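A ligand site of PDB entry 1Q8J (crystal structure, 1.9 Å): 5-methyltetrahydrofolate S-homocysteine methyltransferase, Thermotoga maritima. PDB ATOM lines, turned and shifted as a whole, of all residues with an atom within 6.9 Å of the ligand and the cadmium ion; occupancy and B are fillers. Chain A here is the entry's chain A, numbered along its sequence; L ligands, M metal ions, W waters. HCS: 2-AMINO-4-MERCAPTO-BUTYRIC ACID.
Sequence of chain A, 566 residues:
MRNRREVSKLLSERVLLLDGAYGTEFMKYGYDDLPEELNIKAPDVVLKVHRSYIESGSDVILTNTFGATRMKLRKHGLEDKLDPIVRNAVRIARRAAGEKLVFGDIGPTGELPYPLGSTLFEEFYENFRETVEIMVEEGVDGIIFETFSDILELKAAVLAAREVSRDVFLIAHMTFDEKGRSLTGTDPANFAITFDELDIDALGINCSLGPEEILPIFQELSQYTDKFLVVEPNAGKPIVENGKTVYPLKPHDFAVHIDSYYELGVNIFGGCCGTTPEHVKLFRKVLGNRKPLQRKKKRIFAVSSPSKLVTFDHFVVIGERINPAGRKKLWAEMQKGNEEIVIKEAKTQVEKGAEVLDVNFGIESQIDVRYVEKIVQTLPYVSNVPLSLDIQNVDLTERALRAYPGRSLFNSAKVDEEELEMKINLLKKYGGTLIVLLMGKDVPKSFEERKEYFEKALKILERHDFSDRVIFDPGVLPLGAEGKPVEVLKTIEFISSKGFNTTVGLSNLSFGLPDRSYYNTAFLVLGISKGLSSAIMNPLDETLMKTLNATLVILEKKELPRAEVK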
ATOM      1  N   ASP A  19     -13.975 -15.560  -9.697  1.00  0.00           N
ATOM      2  CA  ASP A  19     -15.363 -15.120  -9.674  1.00  0.00           C
ATOM      3  C   ASP A  19     -15.466 -13.597  -9.547  1.00  0.00           C
ATOM      4  O   ASP A  19     -14.469 -12.899  -9.688  1.00  0.00           O
ATOM      5  CB  ASP A  19     -16.127 -15.818  -8.551  1.00  0.00           C
ATOM      6  CG  ASP A  19     -15.432 -15.657  -7.173  1.00  0.00           C
ATOM      7  OD1 ASP A  19     -15.895 -16.303  -6.234  1.00  0.00           O
ATOM      8  OD2 ASP A  19     -14.437 -14.906  -7.061  1.00  0.00           O
ATOM      9  N   GLY A  20     -16.663 -13.093  -9.288  1.00  0.00           N
ATOM     10  CA  GLY A  20     -16.874 -11.647  -9.170  1.00  0.00           C
ATOM     11  C   GLY A  20     -16.989 -11.264  -7.698  1.00  0.00           C
ATOM     12  O   GLY A  20     -16.491 -11.976  -6.847  1.00  0.00           O
ATOM     13  N   ALA A  21     -17.657 -10.143  -7.413  1.00  0.00           N
ATOM     14  CA  ALA A  21     -17.835  -9.647  -6.039  1.00  0.00           C
ATOM     15  C   ALA A  21     -18.945 -10.352  -5.273  1.00  0.00           C
ATOM     16  O   ALA A  21     -19.908 -10.880  -5.858  1.00  0.00           O
ATOM     17  CB  ALA A  21     -18.128  -8.105  -6.085  1.00  0.00           C
ATOM     18  N   TYR A  22     -18.818 -10.365  -3.940  1.00  0.00           N
ATOM     19  CA  TYR A  22     -19.856 -10.921  -3.086  1.00  0.00           C
ATOM     20  C   TYR A  22     -20.461  -9.751  -2.266  1.00  0.00           C
ATOM     21  O   TYR A  22     -21.679  -9.585  -2.259  1.00  0.00           O
ATOM     22  CB  TYR A  22     -19.286 -12.008  -2.175  1.00  0.00           C
ATOM     23  CG  TYR A  22     -18.985 -13.277  -2.953  1.00  0.00           C
ATOM     24  CD1 TYR A  22     -17.797 -13.416  -3.663  1.00  0.00           C
ATOM     25  CD2 TYR A  22     -19.934 -14.302  -3.048  1.00  0.00           C
ATOM     26  CE1 TYR A  22     -17.555 -14.539  -4.449  1.00  0.00           C
ATOM     27  CE2 TYR A  22     -19.691 -15.442  -3.833  1.00  0.00           C
ATOM     28  CZ  TYR A  22     -18.499 -15.546  -4.532  1.00  0.00           C
ATOM     29  OH  TYR A  22     -18.230 -16.678  -5.307  1.00  0.00           O
ATOM     30  N   GLY A  23     -19.616  -8.945  -1.635  1.00  0.00           N
ATOM     31  CA  GLY A  23     -20.072  -7.808  -0.855  1.00  0.00           C
ATOM     32  C   GLY A  23     -20.972  -6.907  -1.675  1.00  0.00           C
ATOM     33  O   GLY A  23     -22.120  -6.643  -1.310  1.00  0.00           O
ATOM     34  N   THR A  24     -20.477  -6.430  -2.809  1.00  0.00           N
ATOM     35  CA  THR A  24     -21.315  -5.578  -3.644  1.00  0.00           C
ATOM     36  C   THR A  24     -22.530  -6.266  -4.299  1.00  0.00           C
ATOM     37  O   THR A  24     -23.329  -5.584  -4.984  1.00  0.00           O
ATOM     38  CB  THR A  24     -20.478  -4.901  -4.714  1.00  0.00           C
ATOM     39  OG1 THR A  24     -19.891  -5.899  -5.555  1.00  0.00           O
ATOM     40  CG2 THR A  24     -19.366  -4.064  -4.064  1.00  0.00           C
ATOM     41  N   PHE A  26     -24.649  -8.996  -2.553  1.00  0.00           N
ATOM     42  CA  PHE A  26     -25.686  -9.327  -1.594  1.00  0.00           C
ATOM     43  C   PHE A  26     -26.835  -8.304  -1.475  1.00  0.00           C
ATOM     44  O   PHE A  26     -27.983  -8.680  -1.277  1.00  0.00           O
ATOM     45  CB  PHE A  26     -25.044  -9.604  -0.228  1.00  0.00           C
ATOM     46  CG  PHE A  26     -24.240 -10.903  -0.187  1.00  0.00           C
ATOM     47  CD1 PHE A  26     -24.772 -12.094  -0.687  1.00  0.00           C
ATOM     48  CD2 PHE A  26     -22.948 -10.928   0.358  1.00  0.00           C
ATOM     49  CE1 PHE A  26     -24.040 -13.293  -0.645  1.00  0.00           C
ATOM     50  CE2 PHE A  26     -22.218 -12.104   0.407  1.00  0.00           C
ATOM     51  CZ  PHE A  26     -22.757 -13.289  -0.098  1.00  0.00           C
ATOM     52  N   PRO A  35     -21.627  -9.444   5.162  1.00  0.00           N
ATOM     53  CA  PRO A  35     -21.514 -10.685   4.395  1.00  0.00           C
ATOM     54  C   PRO A  35     -21.314 -11.994   5.178  1.00  0.00           C
ATOM     55  O   PRO A  35     -22.049 -12.970   4.976  1.00  0.00           O
ATOM     56  CB  PRO A  35     -20.356 -10.374   3.445  1.00  0.00           C
ATOM     57  CG  PRO A  35     -20.558  -8.943   3.142  1.00  0.00           C
ATOM     58  CD  PRO A  35     -20.885  -8.342   4.512  1.00  0.00           C
ATOM     59  N   GLU A  36     -20.345 -12.017   6.091  1.00  0.00           N
ATOM     60  CA  GLU A  36     -20.077 -13.236   6.853  1.00  0.00           C
ATOM     61  C   GLU A  36     -21.247 -13.769   7.655  1.00  0.00           C
ATOM     62  O   GLU A  36     -21.367 -14.977   7.873  1.00  0.00           O
ATOM     63  CB  GLU A  36     -18.878 -13.022   7.785  1.00  0.00           C
ATOM     64  CG  GLU A  36     -17.584 -12.785   7.029  1.00  0.00           C
ATOM     65  CD  GLU A  36     -17.552 -11.425   6.371  1.00  0.00           C
ATOM     66  OE1 GLU A  36     -16.838 -11.275   5.360  1.00  0.00           O
ATOM     67  OE2 GLU A  36     -18.239 -10.503   6.860  1.00  0.00           O
ATOM     68  N   LEU A  62     -14.462 -18.014  -4.469  1.00  0.00           N
ATOM     69  CA  LEU A  62     -13.912 -17.679  -3.135  1.00  0.00           C
ATOM     70  C   LEU A  62     -14.942 -17.938  -2.013  1.00  0.00           C
ATOM     71  O   LEU A  62     -16.129 -17.651  -2.184  1.00  0.00           O
ATOM     72  CB  LEU A  62     -13.547 -16.204  -3.087  1.00  0.00           C
ATOM     73  CG  LEU A  62     -12.561 -15.595  -4.093  1.00  0.00           C
ATOM     74  CD1 LEU A  62     -12.501 -14.080  -3.883  1.00  0.00           C
ATOM     75  CD2 LEU A  62     -11.188 -16.183  -3.927  1.00  0.00           C
ATOM     76  N   THR A  63     -14.498 -18.447  -0.843  1.00  0.00           N
ATOM     77  CA  THR A  63     -15.438 -18.643   0.257  1.00  0.00           C
ATOM     78  C   THR A  63     -15.858 -17.244   0.774  1.00  0.00           C
ATOM     79  O   THR A  63     -15.089 -16.260   0.642  1.00  0.00           O
ATOM     80  CB  THR A  63     -14.796 -19.482   1.395  1.00  0.00           C
ATOM     81  OG1 THR A  63     -13.578 -18.864   1.799  1.00  0.00           O
ATOM     82  CG2 THR A  63     -14.469 -20.909   0.898  1.00  0.00           C
ATOM     83  N   ASN A  64     -17.049 -17.152   1.343  1.00  0.00           N
ATOM     84  CA  ASN A  64     -17.620 -15.898   1.846  1.00  0.00           C
ATOM     85  C   ASN A  64     -17.079 -15.675   3.279  1.00  0.00           C
ATOM     86  O   ASN A  64     -17.843 -15.634   4.236  1.00  0.00           O
ATOM     87  CB  ASN A  64     -19.128 -16.030   1.835  1.00  0.00           C
ATOM     88  CG  ASN A  64     -19.860 -14.782   2.318  1.00  0.00           C
ATOM     89  OD1 ASN A  64     -19.435 -13.674   2.111  1.00  0.00           O
ATOM     90  ND2 ASN A  64     -21.027 -14.999   2.938  1.00  0.00           N
ATOM     91  N   PHE A  66     -14.235 -13.244   3.771  1.00  0.00           N
ATOM     92  CA  PHE A  66     -13.336 -12.131   3.726  1.00  0.00           C
ATOM     93  C   PHE A  66     -13.069 -11.489   5.108  1.00  0.00           C
ATOM     94  O   PHE A  66     -11.933 -11.187   5.425  1.00  0.00           O
ATOM     95  CB  PHE A  66     -13.855 -11.072   2.755  1.00  0.00           C
ATOM     96  CG  PHE A  66     -12.959  -9.888   2.628  1.00  0.00           C
ATOM     97  CD1 PHE A  66     -13.296  -8.675   3.241  1.00  0.00           C
ATOM     98  CD2 PHE A  66     -11.780  -9.965   1.894  1.00  0.00           C
ATOM     99  CE1 PHE A  66     -12.471  -7.552   3.150  1.00  0.00           C
ATOM    100  CE2 PHE A  66     -10.950  -8.877   1.780  1.00  0.00           C
ATOM    101  CZ  PHE A  66     -11.275  -7.652   2.410  1.00  0.00           C
ATOM    102  N   ASP A 105     -11.052 -17.523   1.300  1.00  0.00           N
ATOM    103  CA  ASP A 105     -10.813 -16.100   1.151  1.00  0.00           C
ATOM    104  C   ASP A 105     -10.628 -15.411   2.535  1.00  0.00           C
ATOM    105  O   ASP A 105     -11.514 -15.494   3.377  1.00  0.00           O
ATOM    106  CB  ASP A 105     -12.036 -15.506   0.430  1.00  0.00           C
ATOM    107  CG  ASP A 105     -11.918 -14.028   0.167  1.00  0.00           C
ATOM    108  OD1 ASP A 105     -10.816 -13.539  -0.152  1.00  0.00           O
ATOM    109  OD2 ASP A 105     -12.961 -13.341   0.258  1.00  0.00           O
ATOM    110  N   PRO A 108      -7.879  -8.536   5.416  1.00  0.00           N
ATOM    111  CA  PRO A 108      -7.185  -7.996   6.602  1.00  0.00           C
ATOM    112  C   PRO A 108      -8.106  -7.688   7.785  1.00  0.00           C
ATOM    113  O   PRO A 108      -9.334  -7.828   7.698  1.00  0.00           O
ATOM    114  CB  PRO A 108      -6.463  -6.763   6.052  1.00  0.00           C
ATOM    115  CG  PRO A 108      -7.401  -6.280   4.925  1.00  0.00           C
ATOM    116  CD  PRO A 108      -8.010  -7.538   4.325  1.00  0.00           C
ATOM    117  N   GLU A 146      -6.712 -11.629   0.373  1.00  0.00           N
ATOM    118  CA  GLU A 146      -7.169 -10.520  -0.474  1.00  0.00           C
ATOM    119  C   GLU A 146      -7.137  -9.142   0.171  1.00  0.00           C
ATOM    120  O   GLU A 146      -7.353  -9.035   1.368  1.00  0.00           O
ATOM    121  CB  GLU A 146      -8.622 -10.726  -0.891  1.00  0.00           C
ATOM    122  CG  GLU A 146      -8.860 -11.613  -2.103  1.00  0.00           C
ATOM    123  CD  GLU A 146     -10.331 -11.630  -2.542  1.00  0.00           C
ATOM    124  OE1 GLU A 146     -11.214 -11.863  -1.698  1.00  0.00           O
ATOM    125  OE2 GLU A 146     -10.613 -11.419  -3.760  1.00  0.00           O
ATOM    126  N   THR A 147      -6.876  -8.128  -0.654  1.00  0.00           N
ATOM    127  CA  THR A 147      -6.959  -6.728  -0.224  1.00  0.00           C
ATOM    128  C   THR A 147      -6.072  -6.274   0.945  1.00  0.00           C
ATOM    129  O   THR A 147      -6.481  -5.422   1.749  1.00  0.00           O
ATOM    130  CB  THR A 147      -8.429  -6.433   0.142  1.00  0.00           C
ATOM    131  OG1 THR A 147      -9.278  -7.254  -0.657  1.00  0.00           O
ATOM    132  CG2 THR A 147      -8.800  -4.918  -0.100  1.00  0.00           C
ATOM    133  N   ASN A 206      -5.752  -6.882  -6.014  1.00  0.00           N
ATOM    134  CA  ASN A 206      -7.179  -6.808  -6.185  1.00  0.00           C
ATOM    135  C   ASN A 206      -7.696  -5.520  -5.546  1.00  0.00           C
ATOM    136  O   ASN A 206      -7.014  -4.923  -4.701  1.00  0.00           O
ATOM    137  CB  ASN A 206      -7.937  -8.007  -5.591  1.00  0.00           C
ATOM    138  CG  ASN A 206      -7.937  -8.019  -4.062  1.00  0.00           C
ATOM    139  OD1 ASN A 206      -6.920  -8.296  -3.429  1.00  0.00           O
ATOM    140  ND2 ASN A 206      -9.090  -7.709  -3.466  1.00  0.00           N
ATOM    141  N   CYS A 207      -8.871  -5.084  -5.997  1.00  0.00           N
ATOM    142  CA  CYS A 207      -9.558  -3.914  -5.420  1.00  0.00           C
ATOM    143  C   CYS A 207      -8.881  -2.557  -5.627  1.00  0.00           C
ATOM    144  O   CYS A 207      -7.866  -2.411  -6.306  1.00  0.00           O
ATOM    145  CB  CYS A 207      -9.783  -4.162  -3.897  1.00  0.00           C
ATOM    146  SG  CYS A 207     -11.177  -3.251  -3.117  1.00  0.00           S
ATOM    147  N   SER A 208      -9.513  -1.547  -5.046  1.00  0.00           N
ATOM    148  CA  SER A 208      -9.047  -0.150  -5.100  1.00  0.00           C
ATOM    149  C   SER A 208      -9.099   0.570  -6.421  1.00  0.00           C
ATOM    150  O   SER A 208      -9.396   1.765  -6.453  1.00  0.00           O
ATOM    151  CB  SER A 208      -7.609   0.008  -4.572  1.00  0.00           C
ATOM    152  OG  SER A 208      -7.529  -0.214  -3.185  1.00  0.00           O
ATOM    153  N   GLU A 232      -7.684  -9.033  -9.733  1.00  0.00           N
ATOM    154  CA  GLU A 232      -9.099  -8.891  -9.597  1.00  0.00           C
ATOM    155  C   GLU A 232      -9.384  -7.392  -9.481  1.00  0.00           C
ATOM    156  O   GLU A 232      -9.472  -6.880  -8.373  1.00  0.00           O
ATOM    157  CB  GLU A 232      -9.670  -9.569  -8.344  1.00  0.00           C
ATOM    158  CG  GLU A 232      -9.530 -11.075  -8.287  1.00  0.00           C
ATOM    159  CD  GLU A 232      -9.904 -11.601  -6.915  1.00  0.00           C
ATOM    160  OE1 GLU A 232     -10.937 -12.268  -6.792  1.00  0.00           O
ATOM    161  OE2 GLU A 232      -9.139 -11.328  -5.958  1.00  0.00           O
ATOM    162  N   ASN A 234     -11.484  -3.783  -9.649  1.00  0.00           N
ATOM    163  CA  ASN A 234     -12.839  -3.350  -9.322  1.00  0.00           C
ATOM    164  C   ASN A 234     -13.434  -3.017 -10.697  1.00  0.00           C
ATOM    165  O   ASN A 234     -12.689  -2.739 -11.624  1.00  0.00           O
ATOM    166  CB  ASN A 234     -12.825  -2.052  -8.515  1.00  0.00           C
ATOM    167  CG  ASN A 234     -12.610  -2.295  -7.040  1.00  0.00           C
ATOM    168  OD1 ASN A 234     -12.701  -3.432  -6.592  1.00  0.00           O
ATOM    169  ND2 ASN A 234     -12.344  -1.238  -6.288  1.00  0.00           N
ATOM    170  N   TYR A 247     -20.006   1.209  -9.200  1.00  0.00           N
ATOM    171  CA  TYR A 247     -18.866   0.801 -10.015  1.00  0.00           C
ATOM    172  C   TYR A 247     -19.483   0.772 -11.407  1.00  0.00           C
ATOM    173  O   TYR A 247     -20.200  -0.146 -11.753  1.00  0.00           O
ATOM    174  CB  TYR A 247     -18.421  -0.583  -9.545  1.00  0.00           C
ATOM    175  CG  TYR A 247     -17.864  -0.551  -8.127  1.00  0.00           C
ATOM    176  CD1 TYR A 247     -16.544  -0.142  -7.876  1.00  0.00           C
ATOM    177  CD2 TYR A 247     -18.651  -0.892  -7.029  1.00  0.00           C
ATOM    178  CE1 TYR A 247     -16.040  -0.090  -6.584  1.00  0.00           C
ATOM    179  CE2 TYR A 247     -18.142  -0.834  -5.716  1.00  0.00           C
ATOM    180  CZ  TYR A 247     -16.845  -0.429  -5.517  1.00  0.00           C
ATOM    181  OH  TYR A 247     -16.324  -0.378  -4.248  1.00  0.00           O
ATOM    182  N   GLY A 271     -12.699 -10.583 -10.875  1.00  0.00           N
ATOM    183  CA  GLY A 271     -13.036  -9.190 -10.595  1.00  0.00           C
ATOM    184  C   GLY A 271     -13.359  -9.018  -9.107  1.00  0.00           C
ATOM    185  O   GLY A 271     -13.776  -9.976  -8.467  1.00  0.00           O
ATOM    186  N   CYS A 272     -13.147  -7.812  -8.568  1.00  0.00           N
ATOM    187  CA  CYS A 272     -13.467  -7.545  -7.167  1.00  0.00           C
ATOM    188  C   CYS A 272     -14.753  -6.664  -7.139  1.00  0.00           C
ATOM    189  O   CYS A 272     -15.573  -6.713  -8.074  1.00  0.00           O
ATOM    190  CB  CYS A 272     -12.310  -6.812  -6.467  1.00  0.00           C
ATOM    191  SG  CYS A 272     -12.272  -7.161  -4.656  1.00  0.00           S
ATOM    192  N   CYS A 273     -14.906  -5.864  -6.087  1.00  0.00           N
ATOM    193  CA  CYS A 273     -16.083  -4.998  -5.928  1.00  0.00           C
ATOM    194  C   CYS A 273     -16.674  -4.413  -7.256  1.00  0.00           C
ATOM    195  O   CYS A 273     -15.975  -3.849  -8.068  1.00  0.00           O
ATOM    196  CB  CYS A 273     -15.721  -3.869  -4.922  1.00  0.00           C
ATOM    197  SG  CYS A 273     -15.233  -4.572  -3.275  1.00  0.00           S
ATOM    198  N   GLY A 274     -17.973  -4.598  -7.448  1.00  0.00           N
ATOM    199  CA  GLY A 274     -18.649  -4.046  -8.611  1.00  0.00           C
ATOM    200  C   GLY A 274     -18.815  -5.029  -9.763  1.00  0.00           C
ATOM    201  O   GLY A 274     -19.612  -4.793 -10.699  1.00  0.00           O
HETATM  202  N   HCS L   1     -13.864 -11.303  -1.830  1.00  0.00           N
HETATM  203  CA  HCS L   1     -14.395 -10.075  -1.210  1.00  0.00           C
HETATM  204  CB  HCS L   1     -13.431  -8.905  -1.506  1.00  0.00           C
HETATM  205  CG  HCS L   1     -13.685  -7.685  -0.606  1.00  0.00           C
HETATM  206  SD  HCS L   1     -12.412  -6.385  -0.800  1.00  0.00           S
HETATM  207  C   HCS L   1     -15.844  -9.794  -1.737  1.00  0.00           C
HETATM  208  OXT HCS L   1     -16.670  -9.306  -0.921  1.00  0.00           O
HETATM  209  O   HCS L   1     -16.079 -10.054  -2.939  1.00  0.00           O
HETATM  210 CD    CD M   1     -12.873  -5.344  -3.153  1.00  0.00          CD
HETATM  211  O   HOH W   1     -15.336 -13.197  -0.592  1.00  0.00           O
HETATM  212  O   HOH W   2     -13.010 -10.674  -4.609  1.00  0.00           O
HETATM  213  O   HOH W   3     -17.751  -6.908  -2.639  1.00  0.00           O
HETATM  214  O   HOH W   4     -17.034  -9.614   1.584  1.00  0.00           O
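The side-chain carboxylate (OD2) of Asp 105 is in salt-bridge range of a nitrogen (N) of the ligand (3.1 Å). A sulfur (SD) of the ligand lies close to the side-chain hydroxyl (OG1) of Thr 147 (3.3 Å). The backbone NH of Gly 23 sits at hydrogen-bond distance from an oxygen (OXT) of the ligand. The side-chain carboxylate (OE1) of Glu 146 is in salt-bridge range of a nitrogen (N) of the ligand, 2.7 Å away. N of Tyr 22 sits at hydrogen-bond distance from O of the ligand, 2.9 Å away.
OD1 of Asp 19 sits at hydrogen-bond distance from OH of Tyr 22. N of Cys 273 sits at hydrogen-bond distance from OD1 of Asn 234 (3.3 Å). The backbone NH (N) of Cys 207 is in hydrogen-bond range of the backbone carbonyl oxygen (O) of Glu 232, 3.0 Å away. The side-chain carboxylate (OE2) of Glu 146 lies close to the side-chain carboxylate (OE2) of Glu 232 (2.6 Å). The backbone NH (N) of Leu 62 sits at hydrogen-bond distance from the side-chain carboxylate (OD1) of Asp 19 (2.8 Å). SG of Cys 272 lies close to ND2 of Asn 206 (3.4 Å). The side-chain hydroxyl of Thr 63 lies within hydrogen-bond range of the backbone NH of Asp 105 (2.9 Å). The side-chain sulfur (SG) of Cys 207 sits close to the side-chain amide oxygen (OD1) of Asn 234.
CA of Ala 21 touches O of the ligand, 3.6 Å away. Leu 62 touches the ligand (CD1 to N, 3.7 Å). CZ of Phe 66 touches SD of the ligand, at 3.6 Å. Of the 27 residues printed, 9 come within 4 Å of the ligand. Along chain A the residues within 4 Å of the ligand span positions 21 to 272. The nearest printed residue that does not touch the ligand is Cys 207 (4.1 Å).
Residues that only touch the cadmium ion: Asn 234. Along chain A the residues within 4 Å of the cadmium ion span positions 207 to 273. The nearest printed residue that does not touch the cadmium ion is Asn 206 (4.5 Å).
The cadmium ion is bound by the side-chain sulfur (SG) of Cys 272 (2.4 Å), the side-chain sulfur (SG) of Cys 273 (2.5 Å), a sulfur (SD) of the ligand (2.6 Å) and the side-chain sulfur (SG) of Cys 207 (2.7 Å). The cadmium ion has four donor atoms within binding distance.
Water W1 lies within hydrogen-bond range of the side-chain carboxylate of Asp 105 (2.5 Å), a nitrogen (N) of the ligand (2.7 Å) and the backbone carbonyl oxygen of Thr 63 (3.3 Å). Water W2 lies within hydrogen-bond range of OE2 of Glu 146 (2.6 Å), N of the ligand (3.0 Å) and OE1 of Glu 232 (3.4 Å). Water W3 lies within hydrogen-bond range of N of Thr 24 (2.8 Å), N of Gly 23 (2.9 Å) and OXT of the ligand (3.1 Å).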
